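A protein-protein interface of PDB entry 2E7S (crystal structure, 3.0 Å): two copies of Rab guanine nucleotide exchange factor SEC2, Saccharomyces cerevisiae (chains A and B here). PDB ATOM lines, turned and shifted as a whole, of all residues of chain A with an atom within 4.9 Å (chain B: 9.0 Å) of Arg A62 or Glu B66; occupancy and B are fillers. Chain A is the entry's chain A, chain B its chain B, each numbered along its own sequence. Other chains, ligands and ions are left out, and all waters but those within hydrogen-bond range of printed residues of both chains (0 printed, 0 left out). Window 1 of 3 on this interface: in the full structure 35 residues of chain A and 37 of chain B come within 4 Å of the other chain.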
ATOM      1  N   GLU A  58     -10.163  -0.060 -35.135  1.00  0.00           N
ATOM      2  CA  GLU A  58      -9.207  -0.280 -34.062  1.00  0.00           C
ATOM      3  C   GLU A  58      -7.818  -0.466 -34.616  1.00  0.00           C
ATOM      4  O   GLU A  58      -6.845  -0.161 -33.948  1.00  0.00           O
ATOM      5  CB  GLU A  58      -9.557  -1.514 -33.248  1.00  0.00           C
ATOM      6  CG  GLU A  58      -8.660  -1.710 -32.042  1.00  0.00           C
ATOM      7  CD  GLU A  58      -8.882  -0.637 -30.993  1.00  0.00           C
ATOM      8  OE1 GLU A  58      -8.724   0.555 -31.332  1.00  0.00           O
ATOM      9  OE2 GLU A  58      -9.221  -0.981 -29.832  1.00  0.00           O
ATOM     10  N   ASN A  59      -7.711  -0.993 -35.827  1.00  0.00           N
ATOM     11  CA  ASN A  59      -6.401  -1.176 -36.427  1.00  0.00           C
ATOM     12  C   ASN A  59      -6.043   0.049 -37.255  1.00  0.00           C
ATOM     13  O   ASN A  59      -4.891   0.241 -37.626  1.00  0.00           O
ATOM     14  CB  ASN A  59      -6.365  -2.438 -37.287  1.00  0.00           C
ATOM     15  CG  ASN A  59      -5.663  -3.593 -36.594  1.00  0.00           C
ATOM     16  OD1 ASN A  59      -4.472  -3.516 -36.293  1.00  0.00           O
ATOM     17  ND2 ASN A  59      -6.398  -4.670 -36.337  1.00  0.00           N
ATOM     18  N   GLU A  60      -7.038   0.881 -37.541  1.00  0.00           N
ATOM     19  CA  GLU A  60      -6.810   2.106 -38.297  1.00  0.00           C
ATOM     20  C   GLU A  60      -6.466   3.218 -37.303  1.00  0.00           C
ATOM     21  O   GLU A  60      -6.067   4.312 -37.689  1.00  0.00           O
ATOM     22  CB  GLU A  60      -8.058   2.475 -39.091  1.00  0.00           C
ATOM     23  CG  GLU A  60      -7.913   3.746 -39.882  1.00  0.00           C
ATOM     24  CD  GLU A  60      -9.164   4.079 -40.666  1.00  0.00           C
ATOM     25  OE1 GLU A  60     -10.254   4.115 -40.046  1.00  0.00           O
ATOM     26  OE2 GLU A  60      -9.056   4.311 -41.897  1.00  0.00           O
ATOM     27  N   LEU A  61      -6.640   2.917 -36.018  1.00  0.00           N
ATOM     28  CA  LEU A  61      -6.333   3.848 -34.945  1.00  0.00           C
ATOM     29  C   LEU A  61      -4.987   3.499 -34.367  1.00  0.00           C
ATOM     30  O   LEU A  61      -4.368   4.327 -33.711  1.00  0.00           O
ATOM     31  CB  LEU A  61      -7.361   3.782 -33.832  1.00  0.00           C
ATOM     32  CG  LEU A  61      -8.720   4.358 -34.183  1.00  0.00           C
ATOM     33  CD1 LEU A  61      -9.590   4.325 -32.944  1.00  0.00           C
ATOM     34  CD2 LEU A  61      -8.564   5.776 -34.711  1.00  0.00           C
ATOM     35  N   ARG A  62      -4.555   2.259 -34.575  1.00  0.00           N
ATOM     36  CA  ARG A  62      -3.242   1.827 -34.108  1.00  0.00           C
ATOM     37  C   ARG A  62      -2.289   2.420 -35.125  1.00  0.00           C
ATOM     38  O   ARG A  62      -1.121   2.652 -34.837  1.00  0.00           O
ATOM     39  CB  ARG A  62      -3.101   0.303 -34.126  1.00  0.00           C
ATOM     40  CG  ARG A  62      -3.149  -0.358 -32.763  1.00  0.00           C
ATOM     41  CD  ARG A  62      -1.988   0.073 -31.870  1.00  0.00           C
ATOM     42  NE  ARG A  62      -1.960  -0.648 -30.588  1.00  0.00           N
ATOM     43  CZ  ARG A  62      -1.040  -0.486 -29.630  1.00  0.00           C
ATOM     44  NH1 ARG A  62      -0.040   0.385 -29.774  1.00  0.00           N
ATOM     45  NH2 ARG A  62      -1.116  -1.211 -28.520  1.00  0.00           N
ATOM     46  N   THR A  63      -2.817   2.678 -36.320  1.00  0.00           N
ATOM     47  CA  THR A  63      -2.050   3.253 -37.426  1.00  0.00           C
ATOM     48  C   THR A  63      -1.462   4.633 -37.086  1.00  0.00           C
ATOM     49  O   THR A  63      -0.248   4.788 -36.982  1.00  0.00           O
ATOM     50  CB  THR A  63      -2.938   3.390 -38.693  1.00  0.00           C
ATOM     51  OG1 THR A  63      -3.525   2.125 -39.018  1.00  0.00           O
ATOM     52  CG2 THR A  63      -2.112   3.865 -39.870  1.00  0.00           C
ATOM     53  N   LYS A  64      -2.324   5.632 -36.916  1.00  0.00           N
ATOM     54  CA  LYS A  64      -1.868   6.979 -36.600  1.00  0.00           C
ATOM     55  C   LYS A  64      -1.107   7.009 -35.284  1.00  0.00           C
ATOM     56  O   LYS A  64      -0.105   7.705 -35.164  1.00  0.00           O
ATOM     57  CB  LYS A  64      -3.044   7.948 -36.509  1.00  0.00           C
ATOM     58  CG  LYS A  64      -3.851   7.768 -35.252  1.00  0.00           C
ATOM     59  CD  LYS A  64      -4.890   8.844 -35.105  1.00  0.00           C
ATOM     60  CE  LYS A  64      -5.672   8.640 -33.821  1.00  0.00           C
ATOM     61  NZ  LYS A  64      -6.683   9.707 -33.643  1.00  0.00           N
ATOM     62  N   ALA A  65      -1.581   6.264 -34.293  1.00  0.00           N
ATOM     63  CA  ALA A  65      -0.921   6.231 -32.994  1.00  0.00           C
ATOM     64  C   ALA A  65       0.458   5.583 -33.081  1.00  0.00           C
ATOM     65  O   ALA A  65       1.225   5.616 -32.121  1.00  0.00           O
ATOM     66  CB  ALA A  65      -1.786   5.498 -31.985  1.00  0.00           C
ATOM     67  N   GLU A  66       0.771   5.000 -34.234  1.00  0.00           N
ATOM     68  CA  GLU A  66       2.065   4.358 -34.451  1.00  0.00           C
ATOM     69  C   GLU A  66       2.902   5.161 -35.439  1.00  0.00           C
ATOM     70  O   GLU A  66       4.116   5.000 -35.509  1.00  0.00           O
ATOM     71  CB  GLU A  66       1.885   2.943 -34.999  1.00  0.00           C
ATOM     72  CG  GLU A  66       3.192   2.172 -35.182  1.00  0.00           C
ATOM     73  CD  GLU A  66       3.023   0.857 -35.943  1.00  0.00           C
ATOM     74  OE1 GLU A  66       2.693   0.907 -37.152  1.00  0.00           O
ATOM     75  OE2 GLU A  66       3.221  -0.225 -35.335  1.00  0.00           O
ATOM     76  N   GLU B  58      -5.138  -9.193 -28.735  1.00  0.00           N
ATOM     77  CA  GLU B  58      -4.653  -7.892 -29.188  1.00  0.00           C
ATOM     78  C   GLU B  58      -4.529  -6.958 -28.000  1.00  0.00           C
ATOM     79  O   GLU B  58      -3.429  -6.557 -27.640  1.00  0.00           O
ATOM     80  CB  GLU B  58      -5.625  -7.262 -30.188  1.00  0.00           C
ATOM     81  CG  GLU B  58      -5.725  -7.943 -31.539  1.00  0.00           C
ATOM     82  CD  GLU B  58      -6.838  -7.362 -32.408  1.00  0.00           C
ATOM     83  OE1 GLU B  58      -6.837  -6.139 -32.640  1.00  0.00           O
ATOM     84  OE2 GLU B  58      -7.714  -8.129 -32.862  1.00  0.00           O
ATOM     85  N   ASN B  59      -5.670  -6.611 -27.401  1.00  0.00           N
ATOM     86  CA  ASN B  59      -5.728  -5.710 -26.241  1.00  0.00           C
ATOM     87  C   ASN B  59      -4.672  -5.980 -25.157  1.00  0.00           C
ATOM     88  O   ASN B  59      -4.071  -5.042 -24.624  1.00  0.00           O
ATOM     89  CB  ASN B  59      -7.121  -5.767 -25.602  1.00  0.00           C
ATOM     90  CG  ASN B  59      -8.203  -5.190 -26.495  1.00  0.00           C
ATOM     91  OD1 ASN B  59      -9.391  -5.277 -26.181  1.00  0.00           O
ATOM     92  ND2 ASN B  59      -7.797  -4.591 -27.611  1.00  0.00           N
ATOM     93  N   GLU B  60      -4.454  -7.252 -24.831  1.00  0.00           N
ATOM     94  CA  GLU B  60      -3.477  -7.634 -23.815  1.00  0.00           C
ATOM     95  C   GLU B  60      -2.048  -7.293 -24.221  1.00  0.00           C
ATOM     96  O   GLU B  60      -1.307  -6.698 -23.448  1.00  0.00           O
ATOM     97  CB  GLU B  60      -3.569  -9.123 -23.538  1.00  0.00           C
ATOM     98  CG  GLU B  60      -2.503  -9.611 -22.607  1.00  0.00           C
ATOM     99  CD  GLU B  60      -1.937 -10.926 -23.068  1.00  0.00           C
ATOM    100  OE1 GLU B  60      -1.402 -10.967 -24.200  1.00  0.00           O
ATOM    101  OE2 GLU B  60      -2.033 -11.914 -22.305  1.00  0.00           O
ATOM    102  N   LEU B  61      -1.659  -7.692 -25.425  1.00  0.00           N
ATOM    103  CA  LEU B  61      -0.324  -7.396 -25.927  1.00  0.00           C
ATOM    104  C   LEU B  61      -0.225  -5.942 -26.412  1.00  0.00           C
ATOM    105  O   LEU B  61       0.834  -5.497 -26.853  1.00  0.00           O
ATOM    106  CB  LEU B  61       0.028  -8.341 -27.071  1.00  0.00           C
ATOM    107  CG  LEU B  61       0.074  -9.819 -26.707  1.00  0.00           C
ATOM    108  CD1 LEU B  61       0.416 -10.646 -27.941  1.00  0.00           C
ATOM    109  CD2 LEU B  61       1.106 -10.024 -25.622  1.00  0.00           C
ATOM    110  N   ARG B  62      -1.334  -5.209 -26.341  1.00  0.00           N
ATOM    111  CA  ARG B  62      -1.357  -3.810 -26.752  1.00  0.00           C
ATOM    112  C   ARG B  62      -1.359  -2.902 -25.536  1.00  0.00           C
ATOM    113  O   ARG B  62      -1.165  -1.704 -25.666  1.00  0.00           O
ATOM    114  CB  ARG B  62      -2.575  -3.509 -27.622  1.00  0.00           C
ATOM    115  CG  ARG B  62      -2.413  -3.958 -29.058  1.00  0.00           C
ATOM    116  CD  ARG B  62      -3.621  -3.585 -29.895  1.00  0.00           C
ATOM    117  NE  ARG B  62      -3.393  -3.835 -31.317  1.00  0.00           N
ATOM    118  CZ  ARG B  62      -4.269  -3.558 -32.279  1.00  0.00           C
ATOM    119  NH1 ARG B  62      -5.448  -3.020 -31.982  1.00  0.00           N
ATOM    120  NH2 ARG B  62      -3.958  -3.806 -33.543  1.00  0.00           N
ATOM    121  N   THR B  63      -1.586  -3.469 -24.353  1.00  0.00           N
ATOM    122  CA  THR B  63      -1.565  -2.684 -23.119  1.00  0.00           C
ATOM    123  C   THR B  63      -0.169  -2.793 -22.501  1.00  0.00           C
ATOM    124  O   THR B  63       0.204  -1.979 -21.652  1.00  0.00           O
ATOM    125  CB  THR B  63      -2.620  -3.170 -22.105  1.00  0.00           C
ATOM    126  OG1 THR B  63      -3.927  -2.979 -22.656  1.00  0.00           O
ATOM    127  CG2 THR B  63      -2.519  -2.384 -20.803  1.00  0.00           C
ATOM    128  N   LYS B  64       0.594  -3.802 -22.933  1.00  0.00           N
ATOM    129  CA  LYS B  64       1.970  -4.008 -22.464  1.00  0.00           C
ATOM    130  C   LYS B  64       2.863  -3.060 -23.252  1.00  0.00           C
ATOM    131  O   LYS B  64       3.815  -2.505 -22.719  1.00  0.00           O
ATOM    132  CB  LYS B  64       2.440  -5.446 -22.708  1.00  0.00           C
ATOM    133  CG  LYS B  64       1.751  -6.493 -21.858  1.00  0.00           C
ATOM    134  CD  LYS B  64       2.332  -7.863 -22.128  1.00  0.00           C
ATOM    135  CE  LYS B  64       1.664  -8.922 -21.274  1.00  0.00           C
ATOM    136  NZ  LYS B  64       2.263 -10.263 -21.525  1.00  0.00           N
ATOM    137  N   ALA B  65       2.539  -2.886 -24.529  1.00  0.00           N
ATOM    138  CA  ALA B  65       3.287  -2.001 -25.405  1.00  0.00           C
ATOM    139  C   ALA B  65       2.909  -0.544 -25.139  1.00  0.00           C
ATOM    140  O   ALA B  65       3.749   0.340 -25.248  1.00  0.00           O
ATOM    141  CB  ALA B  65       3.018  -2.356 -26.864  1.00  0.00           C
ATOM    142  N   GLU B  66       1.651  -0.294 -24.785  1.00  0.00           N
ATOM    143  CA  GLU B  66       1.187   1.066 -24.506  1.00  0.00           C
ATOM    144  C   GLU B  66       1.683   1.588 -23.164  1.00  0.00           C
ATOM    145  O   GLU B  66       1.936   2.779 -23.011  1.00  0.00           O
ATOM    146  CB  GLU B  66      -0.346   1.132 -24.524  1.00  0.00           C
ATOM    147  CG  GLU B  66      -0.985   1.072 -25.914  1.00  0.00           C
ATOM    148  CD  GLU B  66      -2.520   1.078 -25.870  1.00  0.00           C
ATOM    149  OE1 GLU B  66      -3.108   2.080 -25.400  1.00  0.00           O
ATOM    150  OE2 GLU B  66      -3.140   0.079 -26.306  1.00  0.00           O
ATOM    151  N   GLU B  67       1.823   0.700 -22.191  1.00  0.00           N
ATOM    152  CA  GLU B  67       2.280   1.108 -20.873  1.00  0.00           C
ATOM    153  C   GLU B  67       3.793   0.996 -20.714  1.00  0.00           C
ATOM    154  O   GLU B  67       4.360   1.550 -19.777  1.00  0.00           O
ATOM    155  CB  GLU B  67       1.557   0.293 -19.798  1.00  0.00           C
ATOM    156  CG  GLU B  67       0.031   0.479 -19.819  1.00  0.00           C
ATOM    157  CD  GLU B  67      -0.685  -0.263 -18.692  1.00  0.00           C
ATOM    158  OE1 GLU B  67      -0.517  -1.498 -18.584  1.00  0.00           O
ATOM    159  OE2 GLU B  67      -1.421   0.386 -17.914  1.00  0.00           O
ATOM    160  N   GLU B  68       4.446   0.286 -21.628  1.00  0.00           N
ATOM    161  CA  GLU B  68       5.901   0.140 -21.587  1.00  0.00           C
ATOM    162  C   GLU B  68       6.529   1.182 -22.492  1.00  0.00           C
ATOM    163  O   GLU B  68       7.535   1.782 -22.143  1.00  0.00           O
ATOM    164  CB  GLU B  68       6.329  -1.245 -22.062  1.00  0.00           C
ATOM    165  CG  GLU B  68       7.829  -1.377 -22.299  1.00  0.00           C
ATOM    166  CD  GLU B  68       8.202  -2.681 -22.995  1.00  0.00           C
ATOM    167  OE1 GLU B  68       7.674  -2.939 -24.099  1.00  0.00           O
ATOM    168  OE2 GLU B  68       9.023  -3.449 -22.443  1.00  0.00           O
ATOM    169  N   ALA B  69       5.936   1.385 -23.662  1.00  0.00           N
ATOM    170  CA  ALA B  69       6.444   2.366 -24.597  1.00  0.00           C
ATOM    171  C   ALA B  69       6.136   3.744 -24.059  1.00  0.00           C
ATOM    172  O   ALA B  69       6.500   4.739 -24.670  1.00  0.00           O
ATOM    173  CB  ALA B  69       5.817   2.191 -25.958  1.00  0.00           C
ATOM    174  N   ASP B  70       5.441   3.804 -22.929  1.00  0.00           N
ATOM    175  CA  ASP B  70       5.142   5.084 -22.306  1.00  0.00           C
ATOM    176  C   ASP B  70       6.215   5.286 -21.246  1.00  0.00           C
ATOM    177  O   ASP B  70       6.789   6.372 -21.100  1.00  0.00           O
ATOM    178  CB  ASP B  70       3.774   5.066 -21.642  1.00  0.00           C
ATOM    179  CG  ASP B  70       3.497   6.336 -20.854  1.00  0.00           C
ATOM    180  OD1 ASP B  70       4.194   6.576 -19.845  1.00  0.00           O
ATOM    181  OD2 ASP B  70       2.588   7.100 -21.244  1.00  0.00           O
ATOM    182  N   LYS B  71       6.478   4.212 -20.512  1.00  0.00           N
ATOM    183  CA  LYS B  71       7.492   4.191 -19.462  1.00  0.00           C
ATOM    184  C   LYS B  71       8.842   4.508 -20.105  1.00  0.00           C
ATOM    185  O   LYS B  71       9.585   5.379 -19.658  1.00  0.00           O
ATOM    186  CB  LYS B  71       7.509   2.796 -18.838  1.00  0.00           C
ATOM    187  CG  LYS B  71       8.482   2.566 -17.706  1.00  0.00           C
ATOM    188  CD  LYS B  71       8.347   1.122 -17.236  1.00  0.00           C
ATOM    189  CE  LYS B  71       9.216   0.810 -16.037  1.00  0.00           C
ATOM    190  NZ  LYS B  71       8.958  -0.584 -15.556  1.00  0.00           N
ATOM    191  N   LEU B  72       9.132   3.791 -21.180  1.00  0.00           N
ATOM    192  CA  LEU B  72      10.368   3.960 -21.918  1.00  0.00           C
ATOM    193  C   LEU B  72      10.287   5.168 -22.837  1.00  0.00           C
ATOM    194  O   LEU B  72      11.047   5.272 -23.795  1.00  0.00           O
ATOM    195  CB  LEU B  72      10.633   2.715 -22.753  1.00  0.00           C
ATOM    196  CG  LEU B  72      11.989   2.575 -23.443  1.00  0.00           C
ATOM    197  CD1 LEU B  72      13.002   2.018 -22.447  1.00  0.00           C
ATOM    198  CD2 LEU B  72      11.865   1.637 -24.636  1.00  0.00           C
ATOM    199  N   ASN B  73       9.347   6.066 -22.573  1.00  0.00           N
ATOM    200  CA  ASN B  73       9.214   7.263 -23.389  1.00  0.00           C
ATOM    201  C   ASN B  73       9.054   8.438 -22.464  1.00  0.00           C
ATOM    202  O   ASN B  73       8.953   9.591 -22.883  1.00  0.00           O
ATOM    203  CB  ASN B  73       8.020   7.189 -24.323  1.00  0.00           C
ATOM    204  CG  ASN B  73       8.020   8.314 -25.339  1.00  0.00           C
ATOM    205  OD1 ASN B  73       8.862   8.353 -26.248  1.00  0.00           O
ATOM    206  ND2 ASN B  73       7.083   9.249 -25.183  1.00  0.00           N
ATOM    207  N   LYS B  74       9.001   8.129 -21.185  1.00  0.00           N
ATOM    208  CA  LYS B  74       8.920   9.171 -20.197  1.00  0.00           C
ATOM    209  C   LYS B  74      10.283   9.122 -19.528  1.00  0.00           C
ATOM    210  O   LYS B  74      10.616   9.967 -18.692  1.00  0.00           O
ATOM    211  CB  LYS B  74       7.784   8.902 -19.219  1.00  0.00           C
ATOM    212  CG  LYS B  74       6.407   9.003 -19.875  1.00  0.00           C
ATOM    213  CD  LYS B  74       6.200  10.351 -20.579  1.00  0.00           C
ATOM    214  CE  LYS B  74       4.822  10.443 -21.234  1.00  0.00           C
ATOM    215  NZ  LYS B  74       4.564  11.774 -21.851  1.00  0.00           N
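The side-chain carboxylate of Glu B58 lies within salt-bridge range of the guanidinium group of Arg B62 (3.5 Å). O of Asn A59 is in hydrogen-bond range of OG1 of Thr A63, at 2.7 Å. O of Arg B62 sits close to OE2 of Glu B66.
OE2 of Glu B66 lies within salt-bridge range of NH2 of Arg A62 (3.3 Å). The side-chain amide oxygen of Asn A59 is in hydrogen-bond range of the guanidinium group of Arg B62, at 2.8 Å. The guanidinium group (NH2) of Arg A62 sits close to the backbone carbonyl oxygen (O) of Arg B62, 2.9 Å away.
Among the printed residues, pairs that only touch across the chains: Glu A58 with Arg B62.
Of the 17 printed residues of chain B, 2 touch a printed residue of chain A. Printed residues of chain B that touch a printed residue of chain A: Arg B62 and Glu B66. Among the printed residues, 4 pairs touch across the chains.
Glu A58 touches Arg B62, but with the chains exchanged Arg A62 does not touch Glu B58 (5.9 Å). Asn A59 touches Arg B62, but with the chains exchanged Arg A62 does not touch Asn B59 (6.2 Å). Arg A62 touches its own counterpart, Arg B62. Arg A62 touches Glu B66, but with the chains exchanged Glu A66 does not touch Arg B62 (8.2 Å).
Printed residues of chain B within 4 Å of Asn A59: Arg B62 (2.8 Å). Of the printed residues of chain B, Arg A62 touches Arg B62 and Glu B66. Lys A64 touches none of the printed residues of chain B. Ala A65 touches none of the printed residues of chain B. Of the printed residues of chain A, Arg B62 touches Glu A58 (3.5 Å), Asn A59 (2.8 Å) and Arg A62 (2.9 Å).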
